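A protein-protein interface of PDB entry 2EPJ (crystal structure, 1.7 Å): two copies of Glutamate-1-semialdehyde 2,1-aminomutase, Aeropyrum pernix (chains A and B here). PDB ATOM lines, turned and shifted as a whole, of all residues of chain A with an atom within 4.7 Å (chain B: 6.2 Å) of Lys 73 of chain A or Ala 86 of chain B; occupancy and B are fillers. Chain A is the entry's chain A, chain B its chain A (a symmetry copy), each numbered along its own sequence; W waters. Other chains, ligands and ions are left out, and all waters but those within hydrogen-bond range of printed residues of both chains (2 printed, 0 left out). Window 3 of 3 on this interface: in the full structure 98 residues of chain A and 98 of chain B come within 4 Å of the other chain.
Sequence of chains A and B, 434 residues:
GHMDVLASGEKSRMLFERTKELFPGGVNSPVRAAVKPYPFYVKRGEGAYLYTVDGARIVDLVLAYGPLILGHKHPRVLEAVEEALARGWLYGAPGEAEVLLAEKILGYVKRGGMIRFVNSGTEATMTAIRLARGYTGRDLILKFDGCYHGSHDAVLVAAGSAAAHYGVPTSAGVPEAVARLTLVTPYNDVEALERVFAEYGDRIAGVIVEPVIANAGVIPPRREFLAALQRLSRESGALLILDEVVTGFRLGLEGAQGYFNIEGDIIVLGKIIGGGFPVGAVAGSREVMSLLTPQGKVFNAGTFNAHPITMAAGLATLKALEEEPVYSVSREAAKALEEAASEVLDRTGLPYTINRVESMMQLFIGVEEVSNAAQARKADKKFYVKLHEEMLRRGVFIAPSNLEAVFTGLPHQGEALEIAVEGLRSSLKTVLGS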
ATOM      1  N   ARG A  44       0.743 -33.031 -34.461  1.00  0.00           N
ATOM      2  CA  ARG A  44       0.955 -32.243 -33.259  1.00  0.00           C
ATOM      3  C   ARG A  44       2.025 -31.185 -33.472  1.00  0.00           C
ATOM      4  O   ARG A  44       2.682 -31.136 -34.514  1.00  0.00           O
ATOM      5  CB  ARG A  44       1.376 -33.153 -32.099  1.00  0.00           C
ATOM      6  CG  ARG A  44       2.814 -33.655 -32.196  1.00  0.00           C
ATOM      7  CD  ARG A  44       3.109 -34.721 -31.143  1.00  0.00           C
ATOM      8  NE  ARG A  44       4.518 -35.104 -31.138  1.00  0.00           N
ATOM      9  CZ  ARG A  44       5.466 -34.463 -30.462  1.00  0.00           C
ATOM     10  NH1 ARG A  44       5.159 -33.403 -29.724  1.00  0.00           N
ATOM     11  NH2 ARG A  44       6.726 -34.875 -30.531  1.00  0.00           N
ATOM     12  N   GLY A  45       2.186 -30.337 -32.466  1.00  0.00           N
ATOM     13  CA  GLY A  45       3.193 -29.297 -32.516  1.00  0.00           C
ATOM     14  C   GLY A  45       3.799 -29.149 -31.134  1.00  0.00           C
ATOM     15  O   GLY A  45       3.101 -29.294 -30.132  1.00  0.00           O
ATOM     16  N   GLU A  46       5.099 -28.883 -31.074  1.00  0.00           N
ATOM     17  CA  GLU A  46       5.781 -28.695 -29.798  1.00  0.00           C
ATOM     18  C   GLU A  46       7.050 -27.891 -30.026  1.00  0.00           C
ATOM     19  O   GLU A  46       7.860 -28.228 -30.888  1.00  0.00           O
ATOM     20  CB  GLU A  46       6.138 -30.037 -29.148  1.00  0.00           C
ATOM     21  CG  GLU A  46       6.669 -29.874 -27.720  1.00  0.00           C
ATOM     22  CD  GLU A  46       7.030 -31.187 -27.053  1.00  0.00           C
ATOM     23  OE1 GLU A  46       6.479 -32.235 -27.446  1.00  0.00           O
ATOM     24  OE2 GLU A  46       7.858 -31.168 -26.116  1.00  0.00           O
ATOM     25  N   GLY A  71       6.074 -20.239 -29.414  1.00  0.00           N
ATOM     26  CA  GLY A  71       6.271 -21.565 -29.966  1.00  0.00           C
ATOM     27  C   GLY A  71       5.068 -22.435 -29.648  1.00  0.00           C
ATOM     28  O   GLY A  71       4.071 -21.946 -29.118  1.00  0.00           O
ATOM     29  N   HIS A  72       5.160 -23.721 -29.965  1.00  0.00           N
ATOM     30  CA  HIS A  72       4.073 -24.662 -29.717  1.00  0.00           C
ATOM     31  C   HIS A  72       4.083 -25.241 -28.308  1.00  0.00           C
ATOM     32  O   HIS A  72       5.136 -25.572 -27.768  1.00  0.00           O
ATOM     33  CB  HIS A  72       4.149 -25.817 -30.716  1.00  0.00           C
ATOM     34  CG  HIS A  72       3.858 -25.416 -32.127  1.00  0.00           C
ATOM     35  ND1 HIS A  72       2.575 -25.321 -32.623  1.00  0.00           N
ATOM     36  CD2 HIS A  72       4.683 -25.086 -33.149  1.00  0.00           C
ATOM     37  CE1 HIS A  72       2.623 -24.953 -33.891  1.00  0.00           C
ATOM     38  NE2 HIS A  72       3.890 -24.804 -34.235  1.00  0.00           N
ATOM     39  N   LYS A  73       2.897 -25.368 -27.726  1.00  0.00           N
ATOM     40  CA  LYS A  73       2.740 -25.942 -26.399  1.00  0.00           C
ATOM     41  C   LYS A  73       3.783 -25.456 -25.391  1.00  0.00           C
ATOM     42  O   LYS A  73       4.472 -26.259 -24.759  1.00  0.00           O
ATOM     43  CB  LYS A  73       2.784 -27.472 -26.509  1.00  0.00           C
ATOM     44  CG  LYS A  73       2.272 -28.206 -25.282  1.00  0.00           C
ATOM     45  CD  LYS A  73       2.141 -29.704 -25.531  1.00  0.00           C
ATOM     46  CE  LYS A  73       3.484 -30.357 -25.803  1.00  0.00           C
ATOM     47  NZ  LYS A  73       3.346 -31.838 -25.911  1.00  0.00           N
ATOM     48  N   HIS A  74       3.899 -24.139 -25.246  1.00  0.00           N
ATOM     49  CA  HIS A  74       4.848 -23.562 -24.298  1.00  0.00           C
ATOM     50  C   HIS A  74       4.486 -24.130 -22.925  1.00  0.00           C
ATOM     51  O   HIS A  74       3.326 -24.097 -22.526  1.00  0.00           O
ATOM     52  CB  HIS A  74       4.727 -22.035 -24.314  1.00  0.00           C
ATOM     53  CG  HIS A  74       5.730 -21.335 -23.450  1.00  0.00           C
ATOM     54  ND1 HIS A  74       5.564 -21.182 -22.090  1.00  0.00           N
ATOM     55  CD2 HIS A  74       6.919 -20.762 -23.752  1.00  0.00           C
ATOM     56  CE1 HIS A  74       6.607 -20.543 -21.592  1.00  0.00           C
ATOM     57  NE2 HIS A  74       7.444 -20.277 -22.579  1.00  0.00           N
ATOM     58  N   PRO A  75       5.475 -24.670 -22.189  1.00  0.00           N
ATOM     59  CA  PRO A  75       5.264 -25.259 -20.860  1.00  0.00           C
ATOM     60  C   PRO A  75       4.438 -24.437 -19.869  1.00  0.00           C
ATOM     61  O   PRO A  75       3.544 -24.973 -19.207  1.00  0.00           O
ATOM     62  CB  PRO A  75       6.687 -25.502 -20.363  1.00  0.00           C
ATOM     63  CG  PRO A  75       7.429 -25.801 -21.626  1.00  0.00           C
ATOM     64  CD  PRO A  75       6.899 -24.736 -22.565  1.00  0.00           C
ATOM     65  N   LEU A  78       0.894 -24.219 -21.204  1.00  0.00           N
ATOM     66  CA  LEU A  78       0.257 -25.528 -21.097  1.00  0.00           C
ATOM     67  C   LEU A  78      -0.237 -25.756 -19.669  1.00  0.00           C
ATOM     68  O   LEU A  78      -1.376 -26.165 -19.457  1.00  0.00           O
ATOM     69  CB  LEU A  78       1.243 -26.638 -21.472  1.00  0.00           C
ATOM     70  CG  LEU A  78       0.717 -28.064 -21.259  1.00  0.00           C
ATOM     71  CD1 LEU A  78      -0.501 -28.305 -22.141  1.00  0.00           C
ATOM     72  CD2 LEU A  78       1.815 -29.070 -21.574  1.00  0.00           C
ATOM     73  N   VAL B  81     -10.153 -33.442 -24.777  1.00  0.00           N
ATOM     74  CA  VAL B  81      -9.470 -32.157 -24.806  1.00  0.00           C
ATOM     75  C   VAL B  81      -8.067 -32.269 -24.211  1.00  0.00           C
ATOM     76  O   VAL B  81      -7.131 -31.626 -24.688  1.00  0.00           O
ATOM     77  CB  VAL B  81     -10.290 -31.085 -24.055  1.00  0.00           C
ATOM     78  CG1 VAL B  81      -9.495 -29.793 -23.941  1.00  0.00           C
ATOM     79  CG2 VAL B  81     -11.589 -30.825 -24.812  1.00  0.00           C
ATOM     80  N   GLU B  82      -7.917 -33.093 -23.178  1.00  0.00           N
ATOM     81  CA  GLU B  82      -6.610 -33.292 -22.555  1.00  0.00           C
ATOM     82  C   GLU B  82      -5.662 -33.901 -23.580  1.00  0.00           C
ATOM     83  O   GLU B  82      -4.508 -33.486 -23.695  1.00  0.00           O
ATOM     84  CB  GLU B  82      -6.729 -34.219 -21.342  1.00  0.00           C
ATOM     85  CG  GLU B  82      -7.439 -33.588 -20.159  1.00  0.00           C
ATOM     86  CD  GLU B  82      -6.554 -32.629 -19.382  1.00  0.00           C
ATOM     87  OE1 GLU B  82      -5.659 -32.010 -19.992  1.00  0.00           O
ATOM     88  OE2 GLU B  82      -6.763 -32.484 -18.157  1.00  0.00           O
ATOM     89  N   GLU B  83      -6.155 -34.884 -24.328  1.00  0.00           N
ATOM     90  CA  GLU B  83      -5.345 -35.535 -25.350  1.00  0.00           C
ATOM     91  C   GLU B  83      -4.997 -34.542 -26.454  1.00  0.00           C
ATOM     92  O   GLU B  83      -3.866 -34.520 -26.946  1.00  0.00           O
ATOM     93  CB  GLU B  83      -6.094 -36.737 -25.931  1.00  0.00           C
ATOM     94  CG  GLU B  83      -6.108 -37.944 -25.005  1.00  0.00           C
ATOM     95  CD  GLU B  83      -7.054 -39.035 -25.464  1.00  0.00           C
ATOM     96  OE1 GLU B  83      -7.167 -39.253 -26.689  1.00  0.00           O
ATOM     97  OE2 GLU B  83      -7.673 -39.686 -24.596  1.00  0.00           O
ATOM     98  N   ALA B  84      -5.967 -33.714 -26.831  1.00  0.00           N
ATOM     99  CA  ALA B  84      -5.753 -32.708 -27.869  1.00  0.00           C
ATOM    100  C   ALA B  84      -4.748 -31.645 -27.426  1.00  0.00           C
ATOM    101  O   ALA B  84      -3.939 -31.181 -28.229  1.00  0.00           O
ATOM    102  CB  ALA B  84      -7.080 -32.049 -28.245  1.00  0.00           C
ATOM    103  N   LEU B  85      -4.807 -31.253 -26.155  1.00  0.00           N
ATOM    104  CA  LEU B  85      -3.891 -30.243 -25.628  1.00  0.00           C
ATOM    105  C   LEU B  85      -2.446 -30.728 -25.682  1.00  0.00           C
ATOM    106  O   LEU B  85      -1.530 -29.952 -25.949  1.00  0.00           O
ATOM    107  CB  LEU B  85      -4.250 -29.888 -24.181  1.00  0.00           C
ATOM    108  CG  LEU B  85      -5.418 -28.926 -23.965  1.00  0.00           C
ATOM    109  CD1 LEU B  85      -5.719 -28.808 -22.475  1.00  0.00           C
ATOM    110  CD2 LEU B  85      -5.063 -27.555 -24.550  1.00  0.00           C
ATOM    111  N   ALA B  86      -2.250 -32.016 -25.421  1.00  0.00           N
ATOM    112  CA  ALA B  86      -0.917 -32.600 -25.443  1.00  0.00           C
ATOM    113  C   ALA B  86      -0.326 -32.545 -26.852  1.00  0.00           C
ATOM    114  O   ALA B  86       0.891 -32.615 -27.022  1.00  0.00           O
ATOM    115  CB  ALA B  86      -0.971 -34.041 -24.949  1.00  0.00           C
ATOM    116  N   ARG B  87      -1.191 -32.421 -27.859  1.00  0.00           N
ATOM    117  CA  ARG B  87      -0.744 -32.352 -29.251  1.00  0.00           C
ATOM    118  C   ARG B  87      -0.522 -30.912 -29.724  1.00  0.00           C
ATOM    119  O   ARG B  87      -0.251 -30.677 -30.900  1.00  0.00           O
ATOM    120  CB  ARG B  87      -1.775 -33.015 -30.179  1.00  0.00           C
ATOM    121  CG  ARG B  87      -2.051 -34.489 -29.899  1.00  0.00           C
ATOM    122  CD  ARG B  87      -2.893 -35.126 -31.013  1.00  0.00           C
ATOM    123  NE  ARG B  87      -4.224 -34.531 -31.153  1.00  0.00           N
ATOM    124  CZ  ARG B  87      -5.321 -34.977 -30.545  1.00  0.00           C
ATOM    125  NH1 ARG B  87      -5.262 -36.033 -29.745  1.00  0.00           N
ATOM    126  NH2 ARG B  87      -6.483 -34.368 -30.739  1.00  0.00           N
ATOM    127  N   GLY B  88      -0.618 -29.951 -28.813  1.00  0.00           N
ATOM    128  CA  GLY B  88      -0.472 -28.562 -29.219  1.00  0.00           C
ATOM    129  C   GLY B  88      -1.876 -28.116 -29.581  1.00  0.00           C
ATOM    130  O   GLY B  88      -2.674 -28.937 -30.031  1.00  0.00           O
ATOM    131  N   TRP B  89      -2.182 -26.832 -29.419  1.00  0.00           N
ATOM    132  CA  TRP B  89      -3.539 -26.353 -29.676  1.00  0.00           C
ATOM    133  C   TRP B  89      -3.816 -25.458 -30.883  1.00  0.00           C
ATOM    134  O   TRP B  89      -4.953 -25.037 -31.084  1.00  0.00           O
ATOM    135  CB  TRP B  89      -4.069 -25.676 -28.404  1.00  0.00           C
ATOM    136  CG  TRP B  89      -3.128 -24.660 -27.812  1.00  0.00           C
ATOM    137  CD1 TRP B  89      -2.988 -23.355 -28.181  1.00  0.00           C
ATOM    138  CD2 TRP B  89      -2.193 -24.880 -26.749  1.00  0.00           C
ATOM    139  NE1 TRP B  89      -2.023 -22.745 -27.413  1.00  0.00           N
ATOM    140  CE2 TRP B  89      -1.519 -23.660 -26.526  1.00  0.00           C
ATOM    141  CE3 TRP B  89      -1.859 -25.992 -25.964  1.00  0.00           C
ATOM    142  CZ2 TRP B  89      -0.528 -23.516 -25.545  1.00  0.00           C
ATOM    143  CZ3 TRP B  89      -0.871 -25.851 -24.987  1.00  0.00           C
ATOM    144  CH2 TRP B  89      -0.219 -24.621 -24.789  1.00  0.00           C
HETATM  145  O   HOH W   1       2.745 -31.937 -29.009  1.00  0.00           O
HETATM  146  O   HOH W   2       0.375 -25.380 -30.908  1.00  0.00           O
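NZ of Lys 73 of chain A is in salt-bridge range of OE1 of Glu 46 of chain A.
NH1 of Arg 87 of chain B sits close to O of Glu 83 of chain B, at 3.5 Å.
The side-chain carboxylate (OE1) of Glu 46 of chain A lies within salt-bridge range of the guanidinium group (NH1) of Arg 44 of chain A.
Of the 9 printed residues of chain A, 4 touch a printed residue of chain B.
Hydrophobic or aromatic side chains of chain A within 4 Å of the printed part of chain B: Leu 78.
Of the 9 printed residues of chain B, 5 touch a printed residue of chain A.
Hydrophobic or aromatic side chains of chain B within 4 Å of the printed part of chain A: Trp 89.
Among the printed residues, 7 pairs touch across the chains.
The side-chain amino group (NZ) of Lys 73 of chain A sits at hydrogen-bond distance from the backbone carbonyl oxygen (O) of Ala 86 of chain B (2.8 Å).
The backbone NH (N) of Gly 45 of chain A lies within hydrogen-bond range of the backbone carbonyl oxygen (O) of Arg 87 of chain B.
Lys 73 of chain A touches three residues of chain B.
Of the printed residues of chain A, Leu 85 of chain B touches Lys 73.
Ala 86 of chain B touches just one residue of chain A: Lys 73 (2.8 Å).
Of the printed residues of chain A, Arg 87 of chain B touches Arg 44 (3.1 Å) and Gly 45 (2.9 Å).
The nearest printed residue of chain A that does not touch Ala 86 of chain B is Gly 45 of chain A (5.1 Å).
The nearest printed residue of chain B that does not touch Gly 45 of chain A is Ala 86 of chain B (5.1 Å).
Water W2 bridges ND1 of His 72 of chain A and N of Trp 89 of chain B.
Water W1 lies within hydrogen-bond range of the backbone carbonyl oxygen of Ala 86 of chain B (2.8 Å), the backbone carbonyl oxygen of Gly 45 of chain A (2.9 Å), the guanidinium group of Arg 44 of chain A (2.9 Å) and the side-chain amino group of Lys 73 of chain A (3.2 Å).
Among the printed residues, pairs that only touch across the chains: Arg 44 of chain A with Arg 87 of chain B (3.1 Å), Gly 45 of chain A with Gly 88 of chain B (3.8 Å), Lys 73 of chain A with Leu 85 of chain B (3.7 Å), Lys 73 of chain A with Trp 89 of chain B (3.6 Å) and Leu 78 of chain A with Trp 89 of chain B (3.8 Å).
No position is printed for both chains.
Of the 7 pairs that touch across the chains among the printed residues, none has its exchanged pair printed and touching as well.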
